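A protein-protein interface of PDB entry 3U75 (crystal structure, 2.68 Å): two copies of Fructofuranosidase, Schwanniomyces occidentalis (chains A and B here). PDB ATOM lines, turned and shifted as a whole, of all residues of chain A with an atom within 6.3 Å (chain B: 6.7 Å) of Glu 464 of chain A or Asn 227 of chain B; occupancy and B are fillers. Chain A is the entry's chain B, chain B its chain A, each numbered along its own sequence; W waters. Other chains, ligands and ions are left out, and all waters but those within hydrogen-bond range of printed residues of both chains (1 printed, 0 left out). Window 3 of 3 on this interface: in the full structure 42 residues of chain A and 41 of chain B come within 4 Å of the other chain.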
ATOM      1  N   HIS A 341      -1.651  12.954 -22.477  1.00  0.00           N
ATOM      2  CA  HIS A 341      -1.134  13.425 -21.216  1.00  0.00           C
ATOM      3  C   HIS A 341      -1.394  12.451 -20.081  1.00  0.00           C
ATOM      4  O   HIS A 341      -2.526  12.194 -19.729  1.00  0.00           O
ATOM      5  CB  HIS A 341      -1.756  14.777 -20.858  1.00  0.00           C
ATOM      6  CG  HIS A 341      -0.912  15.962 -21.235  1.00  0.00           C
ATOM      7  ND1 HIS A 341      -1.340  16.928 -22.122  1.00  0.00           N
ATOM      8  CD2 HIS A 341       0.327  16.339 -20.837  1.00  0.00           C
ATOM      9  CE1 HIS A 341      -0.401  17.848 -22.254  1.00  0.00           C
ATOM     10  NE2 HIS A 341       0.618  17.517 -21.483  1.00  0.00           N
ATOM     11  N   THR A 342      -0.320  11.933 -19.489  1.00  0.00           N
ATOM     12  CA  THR A 342      -0.413  10.993 -18.363  1.00  0.00           C
ATOM     13  C   THR A 342      -0.274  11.697 -16.996  1.00  0.00           C
ATOM     14  O   THR A 342      -0.826  11.216 -15.991  1.00  0.00           O
ATOM     15  CB  THR A 342       0.623   9.855 -18.492  1.00  0.00           C
ATOM     16  OG1 THR A 342       1.918  10.410 -18.698  1.00  0.00           O
ATOM     17  CG2 THR A 342       0.287   8.945 -19.686  1.00  0.00           C
ATOM     18  N   ASN A 343       0.475  12.809 -16.964  1.00  0.00           N
ATOM     19  CA  ASN A 343       0.418  13.783 -15.869  1.00  0.00           C
ATOM     20  C   ASN A 343       0.139  15.131 -16.495  1.00  0.00           C
ATOM     21  O   ASN A 343      -0.405  15.187 -17.590  1.00  0.00           O
ATOM     22  CB  ASN A 343       1.679  13.789 -15.011  1.00  0.00           C
ATOM     23  CG  ASN A 343       2.963  13.867 -15.835  1.00  0.00           C
ATOM     24  OD1 ASN A 343       3.229  14.868 -16.511  1.00  0.00           O
ATOM     25  ND2 ASN A 343       3.780  12.830 -15.748  1.00  0.00           N
ATOM     26  N   ALA A 344       0.495  16.221 -15.835  1.00  0.00           N
ATOM     27  CA  ALA A 344       0.324  17.540 -16.464  1.00  0.00           C
ATOM     28  C   ALA A 344       1.480  17.973 -17.389  1.00  0.00           C
ATOM     29  O   ALA A 344       1.263  18.752 -18.312  1.00  0.00           O
ATOM     30  CB  ALA A 344       0.082  18.591 -15.423  1.00  0.00           C
ATOM     31  N   SER A 436      -9.899  12.894 -10.166  1.00  0.00           N
ATOM     32  CA  SER A 436      -9.702  12.846 -11.626  1.00  0.00           C
ATOM     33  C   SER A 436      -9.808  11.424 -12.146  1.00  0.00           C
ATOM     34  O   SER A 436      -9.122  11.051 -13.100  1.00  0.00           O
ATOM     35  CB  SER A 436      -8.359  13.467 -12.052  1.00  0.00           C
ATOM     36  OG  SER A 436      -8.335  13.692 -13.448  1.00  0.00           O
ATOM     37  N   TYR A 462      -7.569   6.457 -13.173  1.00  0.00           N
ATOM     38  CA  TYR A 462      -7.105   7.837 -13.197  1.00  0.00           C
ATOM     39  C   TYR A 462      -6.797   8.285 -14.621  1.00  0.00           C
ATOM     40  O   TYR A 462      -6.060   7.628 -15.325  1.00  0.00           O
ATOM     41  CB  TYR A 462      -5.856   7.997 -12.341  1.00  0.00           C
ATOM     42  CG  TYR A 462      -5.296   9.397 -12.361  1.00  0.00           C
ATOM     43  CD1 TYR A 462      -5.720  10.350 -11.435  1.00  0.00           C
ATOM     44  CD2 TYR A 462      -4.348   9.773 -13.316  1.00  0.00           C
ATOM     45  CE1 TYR A 462      -5.217  11.640 -11.469  1.00  0.00           C
ATOM     46  CE2 TYR A 462      -3.842  11.058 -13.351  1.00  0.00           C
ATOM     47  CZ  TYR A 462      -4.276  11.987 -12.427  1.00  0.00           C
ATOM     48  OH  TYR A 462      -3.792  13.275 -12.430  1.00  0.00           O
ATOM     49  N   LEU A 463      -7.371   9.418 -15.023  1.00  0.00           N
ATOM     50  CA  LEU A 463      -7.096  10.014 -16.305  1.00  0.00           C
ATOM     51  C   LEU A 463      -6.848  11.500 -16.156  1.00  0.00           C
ATOM     52  O   LEU A 463      -7.361  12.146 -15.237  1.00  0.00           O
ATOM     53  CB  LEU A 463      -8.242   9.759 -17.273  1.00  0.00           C
ATOM     54  CG  LEU A 463      -8.140   8.354 -17.888  1.00  0.00           C
ATOM     55  CD1 LEU A 463      -9.082   7.396 -17.205  1.00  0.00           C
ATOM     56  CD2 LEU A 463      -8.437   8.402 -19.355  1.00  0.00           C
ATOM     57  N   GLU A 464      -6.020  12.024 -17.053  1.00  0.00           N
ATOM     58  CA  GLU A 464      -5.838  13.456 -17.207  1.00  0.00           C
ATOM     59  C   GLU A 464      -6.981  14.040 -18.060  1.00  0.00           C
ATOM     60  O   GLU A 464      -7.700  13.287 -18.720  1.00  0.00           O
ATOM     61  CB  GLU A 464      -4.486  13.710 -17.859  1.00  0.00           C
ATOM     62  CG  GLU A 464      -3.341  13.402 -16.934  1.00  0.00           C
ATOM     63  CD  GLU A 464      -3.062  14.511 -15.956  1.00  0.00           C
ATOM     64  OE1 GLU A 464      -3.362  15.692 -16.246  1.00  0.00           O
ATOM     65  OE2 GLU A 464      -2.498  14.186 -14.894  1.00  0.00           O
ATOM     66  N   PRO A 465      -7.192  15.376 -18.022  1.00  0.00           N
ATOM     67  CA  PRO A 465      -8.175  15.957 -18.949  1.00  0.00           C
ATOM     68  C   PRO A 465      -7.980  15.561 -20.409  1.00  0.00           C
ATOM     69  O   PRO A 465      -6.844  15.475 -20.877  1.00  0.00           O
ATOM     70  CB  PRO A 465      -7.941  17.458 -18.782  1.00  0.00           C
ATOM     71  CG  PRO A 465      -7.550  17.589 -17.355  1.00  0.00           C
ATOM     72  CD  PRO A 465      -6.873  16.314 -16.928  1.00  0.00           C
ATOM     73  N   LEU A 466      -9.077  15.306 -21.106  1.00  0.00           N
ATOM     74  CA  LEU A 466      -9.065  15.208 -22.560  1.00  0.00           C
ATOM     75  C   LEU A 466      -8.699  16.575 -23.094  1.00  0.00           C
ATOM     76  O   LEU A 466      -7.834  16.704 -23.962  1.00  0.00           O
ATOM     77  CB  LEU A 466     -10.449  14.826 -23.094  1.00  0.00           C
ATOM     78  CG  LEU A 466     -10.730  14.796 -24.599  1.00  0.00           C
ATOM     79  CD1 LEU A 466     -10.056  13.586 -25.269  1.00  0.00           C
ATOM     80  CD2 LEU A 466     -12.222  14.807 -24.892  1.00  0.00           C
ATOM     81  N   ASP A 467      -9.363  17.593 -22.551  1.00  0.00           N
ATOM     82  CA  ASP A 467      -9.150  18.962 -22.974  1.00  0.00           C
ATOM     83  C   ASP A 467      -9.441  19.952 -21.856  1.00  0.00           C
ATOM     84  O   ASP A 467     -10.184  19.659 -20.903  1.00  0.00           O
ATOM     85  CB  ASP A 467     -10.061  19.277 -24.161  1.00  0.00           C
ATOM     86  CG  ASP A 467      -9.380  20.120 -25.222  1.00  0.00           C
ATOM     87  OD1 ASP A 467      -8.398  20.847 -24.931  1.00  0.00           O
ATOM     88  OD2 ASP A 467      -9.843  20.045 -26.366  1.00  0.00           O
ATOM     89  N   TYR A 468      -8.834  21.129 -21.990  1.00  0.00           N
ATOM     90  CA  TYR A 468      -9.189  22.277 -21.164  1.00  0.00           C
ATOM     91  C   TYR A 468      -9.986  23.237 -22.025  1.00  0.00           C
ATOM     92  O   TYR A 468      -9.556  23.608 -23.114  1.00  0.00           O
ATOM     93  CB  TYR A 468      -7.949  22.962 -20.551  1.00  0.00           C
ATOM     94  CG  TYR A 468      -7.082  22.019 -19.746  1.00  0.00           C
ATOM     95  CD1 TYR A 468      -6.103  21.251 -20.382  1.00  0.00           C
ATOM     96  CD2 TYR A 468      -7.250  21.883 -18.363  1.00  0.00           C
ATOM     97  CE1 TYR A 468      -5.310  20.379 -19.679  1.00  0.00           C
ATOM     98  CE2 TYR A 468      -6.454  21.001 -17.631  1.00  0.00           C
ATOM     99  CZ  TYR A 468      -5.483  20.246 -18.301  1.00  0.00           C
ATOM    100  OH  TYR A 468      -4.680  19.340 -17.621  1.00  0.00           O
ATOM    101  N   VAL A 474     -12.266  19.170 -19.199  1.00  0.00           N
ATOM    102  CA  VAL A 474     -13.223  18.462 -20.036  1.00  0.00           C
ATOM    103  C   VAL A 474     -12.860  16.977 -20.101  1.00  0.00           C
ATOM    104  O   VAL A 474     -11.723  16.622 -20.445  1.00  0.00           O
ATOM    105  CB  VAL A 474     -13.266  19.076 -21.469  1.00  0.00           C
ATOM    106  CG1 VAL A 474     -14.233  18.305 -22.375  1.00  0.00           C
ATOM    107  CG2 VAL A 474     -13.619  20.595 -21.413  1.00  0.00           C
ATOM    108  N   PHE A 475     -13.821  16.114 -19.748  1.00  0.00           N
ATOM    109  CA  PHE A 475     -13.611  14.662 -19.803  1.00  0.00           C
ATOM    110  C   PHE A 475     -14.651  14.031 -20.733  1.00  0.00           C
ATOM    111  O   PHE A 475     -15.665  14.664 -21.002  1.00  0.00           O
ATOM    112  CB  PHE A 475     -13.696  14.055 -18.390  1.00  0.00           C
ATOM    113  CG  PHE A 475     -12.499  14.351 -17.496  1.00  0.00           C
ATOM    114  CD1 PHE A 475     -12.427  15.549 -16.776  1.00  0.00           C
ATOM    115  CD2 PHE A 475     -11.454  13.412 -17.355  1.00  0.00           C
ATOM    116  CE1 PHE A 475     -11.322  15.825 -15.950  1.00  0.00           C
ATOM    117  CE2 PHE A 475     -10.344  13.663 -16.537  1.00  0.00           C
ATOM    118  CZ  PHE A 475     -10.273  14.864 -15.833  1.00  0.00           C
ATOM    119  N   ASN A 491     -12.090   9.134 -22.180  1.00  0.00           N
ATOM    120  CA  ASN A 491     -11.459  10.180 -22.978  1.00  0.00           C
ATOM    121  C   ASN A 491     -11.117   9.628 -24.347  1.00  0.00           C
ATOM    122  O   ASN A 491      -9.933   9.468 -24.683  1.00  0.00           O
ATOM    123  CB  ASN A 491     -10.210  10.758 -22.278  1.00  0.00           C
ATOM    124  CG  ASN A 491     -10.549  11.581 -21.044  1.00  0.00           C
ATOM    125  OD1 ASN A 491     -11.683  11.920 -20.794  1.00  0.00           O
ATOM    126  ND2 ASN A 491      -9.546  11.911 -20.281  1.00  0.00           N
ATOM    127  N   ARG B 178      11.504  16.345  -5.994  1.00  0.00           N
ATOM    128  CA  ARG B 178      11.316  16.111  -4.572  1.00  0.00           C
ATOM    129  C   ARG B 178      11.653  14.698  -4.119  1.00  0.00           C
ATOM    130  O   ARG B 178      11.655  13.776  -4.931  1.00  0.00           O
ATOM    131  CB  ARG B 178       9.863  16.455  -4.187  1.00  0.00           C
ATOM    132  CG  ARG B 178       8.826  15.798  -5.071  1.00  0.00           C
ATOM    133  CD  ARG B 178       7.423  15.862  -4.523  1.00  0.00           C
ATOM    134  NE  ARG B 178       6.484  15.186  -5.425  1.00  0.00           N
ATOM    135  CZ  ARG B 178       5.887  15.743  -6.483  1.00  0.00           C
ATOM    136  NH1 ARG B 178       6.082  17.007  -6.825  1.00  0.00           N
ATOM    137  NH2 ARG B 178       5.078  15.023  -7.218  1.00  0.00           N
ATOM    138  N   SER B 198       9.656  14.401 -10.619  1.00  0.00           N
ATOM    139  CA  SER B 198       8.398  13.710 -10.400  1.00  0.00           C
ATOM    140  C   SER B 198       7.575  13.431 -11.635  1.00  0.00           C
ATOM    141  O   SER B 198       7.202  12.294 -11.885  1.00  0.00           O
ATOM    142  CB  SER B 198       7.589  14.456  -9.359  1.00  0.00           C
ATOM    143  OG  SER B 198       8.238  14.314  -8.112  1.00  0.00           O
ATOM    144  N   GLN B 199       7.304  14.466 -12.415  1.00  0.00           N
ATOM    145  CA  GLN B 199       6.455  14.323 -13.604  1.00  0.00           C
ATOM    146  C   GLN B 199       7.233  14.088 -14.905  1.00  0.00           C
ATOM    147  O   GLN B 199       6.668  14.130 -15.989  1.00  0.00           O
ATOM    148  CB  GLN B 199       5.528  15.516 -13.720  1.00  0.00           C
ATOM    149  CG  GLN B 199       4.564  15.581 -12.564  1.00  0.00           C
ATOM    150  CD  GLN B 199       3.492  16.618 -12.758  1.00  0.00           C
ATOM    151  OE1 GLN B 199       2.510  16.670 -12.008  1.00  0.00           O
ATOM    152  NE2 GLN B 199       3.670  17.459 -13.773  1.00  0.00           N
ATOM    153  N   TYR B 201       9.033  11.271 -14.944  1.00  0.00           N
ATOM    154  CA  TYR B 201       9.292   9.855 -14.698  1.00  0.00           C
ATOM    155  C   TYR B 201      10.771   9.560 -14.785  1.00  0.00           C
ATOM    156  O   TYR B 201      11.191   8.652 -15.497  1.00  0.00           O
ATOM    157  CB  TYR B 201       8.567   8.937 -15.684  1.00  0.00           C
ATOM    158  CG  TYR B 201       7.123   9.219 -15.829  1.00  0.00           C
ATOM    159  CD1 TYR B 201       6.652   9.876 -16.957  1.00  0.00           C
ATOM    160  CD2 TYR B 201       6.206   8.844 -14.830  1.00  0.00           C
ATOM    161  CE1 TYR B 201       5.296  10.145 -17.112  1.00  0.00           C
ATOM    162  CE2 TYR B 201       4.837   9.119 -14.973  1.00  0.00           C
ATOM    163  CZ  TYR B 201       4.399   9.767 -16.123  1.00  0.00           C
ATOM    164  OH  TYR B 201       3.073  10.050 -16.292  1.00  0.00           O
ATOM    165  N   TYR B 224       6.055   0.514 -13.633  1.00  0.00           N
ATOM    166  CA  TYR B 224       4.734   1.096 -13.847  1.00  0.00           C
ATOM    167  C   TYR B 224       4.819   2.625 -13.662  1.00  0.00           C
ATOM    168  O   TYR B 224       5.259   3.109 -12.625  1.00  0.00           O
ATOM    169  CB  TYR B 224       3.726   0.451 -12.874  1.00  0.00           C
ATOM    170  CG  TYR B 224       2.317   0.432 -13.397  1.00  0.00           C
ATOM    171  CD1 TYR B 224       1.968  -0.389 -14.462  1.00  0.00           C
ATOM    172  CD2 TYR B 224       1.335   1.245 -12.854  1.00  0.00           C
ATOM    173  CE1 TYR B 224       0.666  -0.401 -14.978  1.00  0.00           C
ATOM    174  CE2 TYR B 224       0.033   1.240 -13.361  1.00  0.00           C
ATOM    175  CZ  TYR B 224      -0.295   0.412 -14.424  1.00  0.00           C
ATOM    176  OH  TYR B 224      -1.586   0.405 -14.937  1.00  0.00           O
ATOM    177  N   TYR B 225       4.440   3.400 -14.671  1.00  0.00           N
ATOM    178  CA  TYR B 225       4.646   4.843 -14.568  1.00  0.00           C
ATOM    179  C   TYR B 225       3.626   5.534 -13.682  1.00  0.00           C
ATOM    180  O   TYR B 225       4.008   6.324 -12.833  1.00  0.00           O
ATOM    181  CB  TYR B 225       4.735   5.522 -15.945  1.00  0.00           C
ATOM    182  CG  TYR B 225       6.090   5.385 -16.631  1.00  0.00           C
ATOM    183  CD1 TYR B 225       6.963   4.355 -16.309  1.00  0.00           C
ATOM    184  CD2 TYR B 225       6.476   6.266 -17.615  1.00  0.00           C
ATOM    185  CE1 TYR B 225       8.162   4.225 -16.934  1.00  0.00           C
ATOM    186  CE2 TYR B 225       7.693   6.136 -18.239  1.00  0.00           C
ATOM    187  CZ  TYR B 225       8.516   5.109 -17.895  1.00  0.00           C
ATOM    188  OH  TYR B 225       9.712   4.964 -18.532  1.00  0.00           O
ATOM    189  N   GLY B 226       2.344   5.228 -13.864  1.00  0.00           N
ATOM    190  CA  GLY B 226       1.303   5.874 -13.108  1.00  0.00           C
ATOM    191  C   GLY B 226       1.298   7.333 -13.492  1.00  0.00           C
ATOM    192  O   GLY B 226       1.607   7.672 -14.601  1.00  0.00           O
ATOM    193  N   ASN B 227       0.963   8.206 -12.553  1.00  0.00           N
ATOM    194  CA  ASN B 227       0.940   9.648 -12.791  1.00  0.00           C
ATOM    195  C   ASN B 227       2.245  10.376 -12.399  1.00  0.00           C
ATOM    196  O   ASN B 227       2.513  11.458 -12.887  1.00  0.00           O
ATOM    197  CB  ASN B 227      -0.271  10.244 -12.048  1.00  0.00           C
ATOM    198  CG  ASN B 227      -0.301  11.758 -12.087  1.00  0.00           C
ATOM    199  OD1 ASN B 227      -0.970  12.370 -12.945  1.00  0.00           O
ATOM    200  ND2 ASN B 227       0.429  12.380 -11.165  1.00  0.00           N
ATOM    201  N   GLN B 228       3.027   9.772 -11.504  1.00  0.00           N
ATOM    202  CA  GLN B 228       4.172  10.403 -10.836  1.00  0.00           C
ATOM    203  C   GLN B 228       5.027   9.356 -10.156  1.00  0.00           C
ATOM    204  O   GLN B 228       4.494   8.477  -9.435  1.00  0.00           O
ATOM    205  CB  GLN B 228       3.729  11.310  -9.703  1.00  0.00           C
ATOM    206  CG  GLN B 228       3.698  12.787  -9.985  1.00  0.00           C
ATOM    207  CD  GLN B 228       2.788  13.497  -8.987  1.00  0.00           C
ATOM    208  OE1 GLN B 228       2.118  12.849  -8.183  1.00  0.00           O
ATOM    209  NE2 GLN B 228       2.755  14.820  -9.045  1.00  0.00           N
ATOM    210  N   TYR B 229       6.344   9.489 -10.377  1.00  0.00           N
ATOM    211  CA  TYR B 229       7.378   8.852  -9.585  1.00  0.00           C
ATOM    212  C   TYR B 229       7.463   9.644  -8.284  1.00  0.00           C
ATOM    213  O   TYR B 229       7.167  10.838  -8.295  1.00  0.00           O
ATOM    214  CB  TYR B 229       8.684   8.985 -10.331  1.00  0.00           C
ATOM    215  CG  TYR B 229       9.011   7.911 -11.363  1.00  0.00           C
ATOM    216  CD1 TYR B 229       8.043   7.021 -11.850  1.00  0.00           C
ATOM    217  CD2 TYR B 229      10.310   7.824 -11.871  1.00  0.00           C
ATOM    218  CE1 TYR B 229       8.373   6.073 -12.795  1.00  0.00           C
ATOM    219  CE2 TYR B 229      10.657   6.883 -12.790  1.00  0.00           C
ATOM    220  CZ  TYR B 229       9.702   6.006 -13.266  1.00  0.00           C
ATOM    221  OH  TYR B 229      10.132   5.072 -14.201  1.00  0.00           O
ATOM    222  N   ILE B 253       4.429   5.281  -6.425  1.00  0.00           N
ATOM    223  CA  ILE B 253       3.667   5.949  -7.447  1.00  0.00           C
ATOM    224  C   ILE B 253       2.254   6.280  -7.002  1.00  0.00           C
ATOM    225  O   ILE B 253       1.523   5.441  -6.481  1.00  0.00           O
ATOM    226  CB  ILE B 253       3.703   5.202  -8.796  1.00  0.00           C
ATOM    227  CG1 ILE B 253       3.096   3.823  -8.679  1.00  0.00           C
ATOM    228  CG2 ILE B 253       5.158   5.042  -9.316  1.00  0.00           C
ATOM    229  CD1 ILE B 253       2.647   3.259  -9.993  1.00  0.00           C
ATOM    230  N   ASN B 254       1.906   7.545  -7.183  1.00  0.00           N
ATOM    231  CA  ASN B 254       0.596   8.040  -6.942  1.00  0.00           C
ATOM    232  C   ASN B 254       0.297   9.305  -7.761  1.00  0.00           C
ATOM    233  O   ASN B 254       1.182  10.124  -7.995  1.00  0.00           O
ATOM    234  CB  ASN B 254       0.447   8.327  -5.467  1.00  0.00           C
ATOM    235  CG  ASN B 254      -0.867   8.958  -5.149  1.00  0.00           C
ATOM    236  OD1 ASN B 254      -1.904   8.282  -5.119  1.00  0.00           O
ATOM    237  ND2 ASN B 254      -0.848  10.268  -4.938  1.00  0.00           N
ATOM    238  N   PRO B 255      -0.952   9.449  -8.247  1.00  0.00           N
ATOM    239  CA  PRO B 255      -1.974   8.404  -8.323  1.00  0.00           C
ATOM    240  C   PRO B 255      -1.737   7.423  -9.487  1.00  0.00           C
ATOM    241  O   PRO B 255      -0.650   7.444 -10.128  1.00  0.00           O
ATOM    242  CB  PRO B 255      -3.252   9.201  -8.516  1.00  0.00           C
ATOM    243  CG  PRO B 255      -2.807  10.434  -9.157  1.00  0.00           C
ATOM    244  CD  PRO B 255      -1.524  10.771  -8.531  1.00  0.00           C
ATOM    245  N   GLY B 256      -2.744   6.572  -9.737  1.00  0.00           N
ATOM    246  CA  GLY B 256      -2.771   5.684 -10.910  1.00  0.00           C
ATOM    247  C   GLY B 256      -2.051   4.379 -10.672  1.00  0.00           C
ATOM    248  O   GLY B 256      -1.528   3.771 -11.599  1.00  0.00           O
ATOM    249  N   SER B 257      -2.005   3.957  -9.413  1.00  0.00           N
ATOM    250  CA  SER B 257      -1.623   2.606  -9.114  1.00  0.00           C
ATOM    251  C   SER B 257      -2.594   1.713  -9.851  1.00  0.00           C
ATOM    252  O   SER B 257      -3.792   2.019  -9.905  1.00  0.00           O
ATOM    253  CB  SER B 257      -1.742   2.313  -7.635  1.00  0.00           C
ATOM    254  OG  SER B 257      -1.609   0.923  -7.433  1.00  0.00           O
HETATM  255  O   HOH W   1      -0.888  15.674 -13.193  1.00  0.00           O
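The backbone carbonyl oxygen (O) of Gln 199 of chain B lies within hydrogen-bond range of the side-chain amide nitrogen (ND2) of Asn 343 of chain A (3.2 Å).
OG1 of Thr 342 of chain A lies within hydrogen-bond range of OH of Tyr 201 of chain B (2.7 Å).
The side-chain amide nitrogen of Asn 343 of chain A sits at hydrogen-bond distance from the side-chain hydroxyl of Tyr 201 of chain B.
The backbone carbonyl oxygen (O) of Thr 342 of chain A lies close to the side-chain amide oxygen (OD1) of Asn 227 of chain B (3.3 Å).
The backbone carbonyl oxygen (O) of Asn 227 of chain B lies close to the side-chain amide nitrogen (ND2) of Asn 343 of chain A (3.4 Å).
OD1 of Asn 227 of chain B sits at hydrogen-bond distance from OH of Tyr 462 of chain A, 3.0 Å away.
The side-chain amide oxygen of Asn 227 of chain B sits close to the side-chain carboxylate of Glu 464 of chain A, 3.1 Å away.
OH of Tyr 201 of chain B lies within hydrogen-bond range of O of Gly 226 of chain B.
ND2 of Asn 227 of chain B sits close to OE1 of Gln 228 of chain B (3.5 Å).
The backbone NH (N) of Asn 227 of chain B lies within hydrogen-bond range of the backbone carbonyl oxygen (O) of Pro 255 of chain B, at 3.0 Å.
A ring nitrogen (NE2) of His 341 of chain A is in hydrogen-bond range of the backbone carbonyl oxygen (O) of Ala 344 of chain A, at 3.5 Å.
The side-chain hydroxyl of Tyr 462 of chain A is in hydrogen-bond range of the side-chain carboxylate of Glu 464 of chain A, at 2.9 Å.
The side-chain amide nitrogen of Asn 491 of chain A lies within hydrogen-bond range of the backbone carbonyl oxygen of Glu 464 of chain A, at 2.8 Å.
Among the printed residues, merely in contact across the chains: Ala 344 of chain A with Gln 199 of chain B (3.98 Å) and Tyr 462 of chain A with Pro 255 of chain B (3.6 Å).
Printed residues of chain B within 4 Å of Thr 342 of chain A: Tyr 201 and Asn 227.
Of the printed residues of chain B, Asn 343 of chain A touches Gln 199 (3.2 Å), Tyr 201 (2.9 Å) and Asn 227 (3.3 Å).
Of the printed residues of chain B, Glu 464 of chain A touches Asn 227.
Asn 227 of chain B touches just these residues of chain A: Thr 342, Asn 343, Tyr 462 and Glu 464.
The nearest printed residue of chain A that does not touch Pro 255 of chain B is Glu 464 of chain A (6.9 Å).
Among the printed residues, no Asp or Glu carboxylate lies within 4 Å of a Lys or Arg side-chain nitrogen of the other chain.
No position is printed for both chains.
Water W1 lies within hydrogen-bond range of the side-chain carboxylate (OE2) of Glu 464 of chain A (2.8 Å), the backbone NH (N) of Ala 344 of chain A (3.0 Å) and the side-chain amide oxygen (OD1) of Asn 227 of chain B (3.3 Å).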
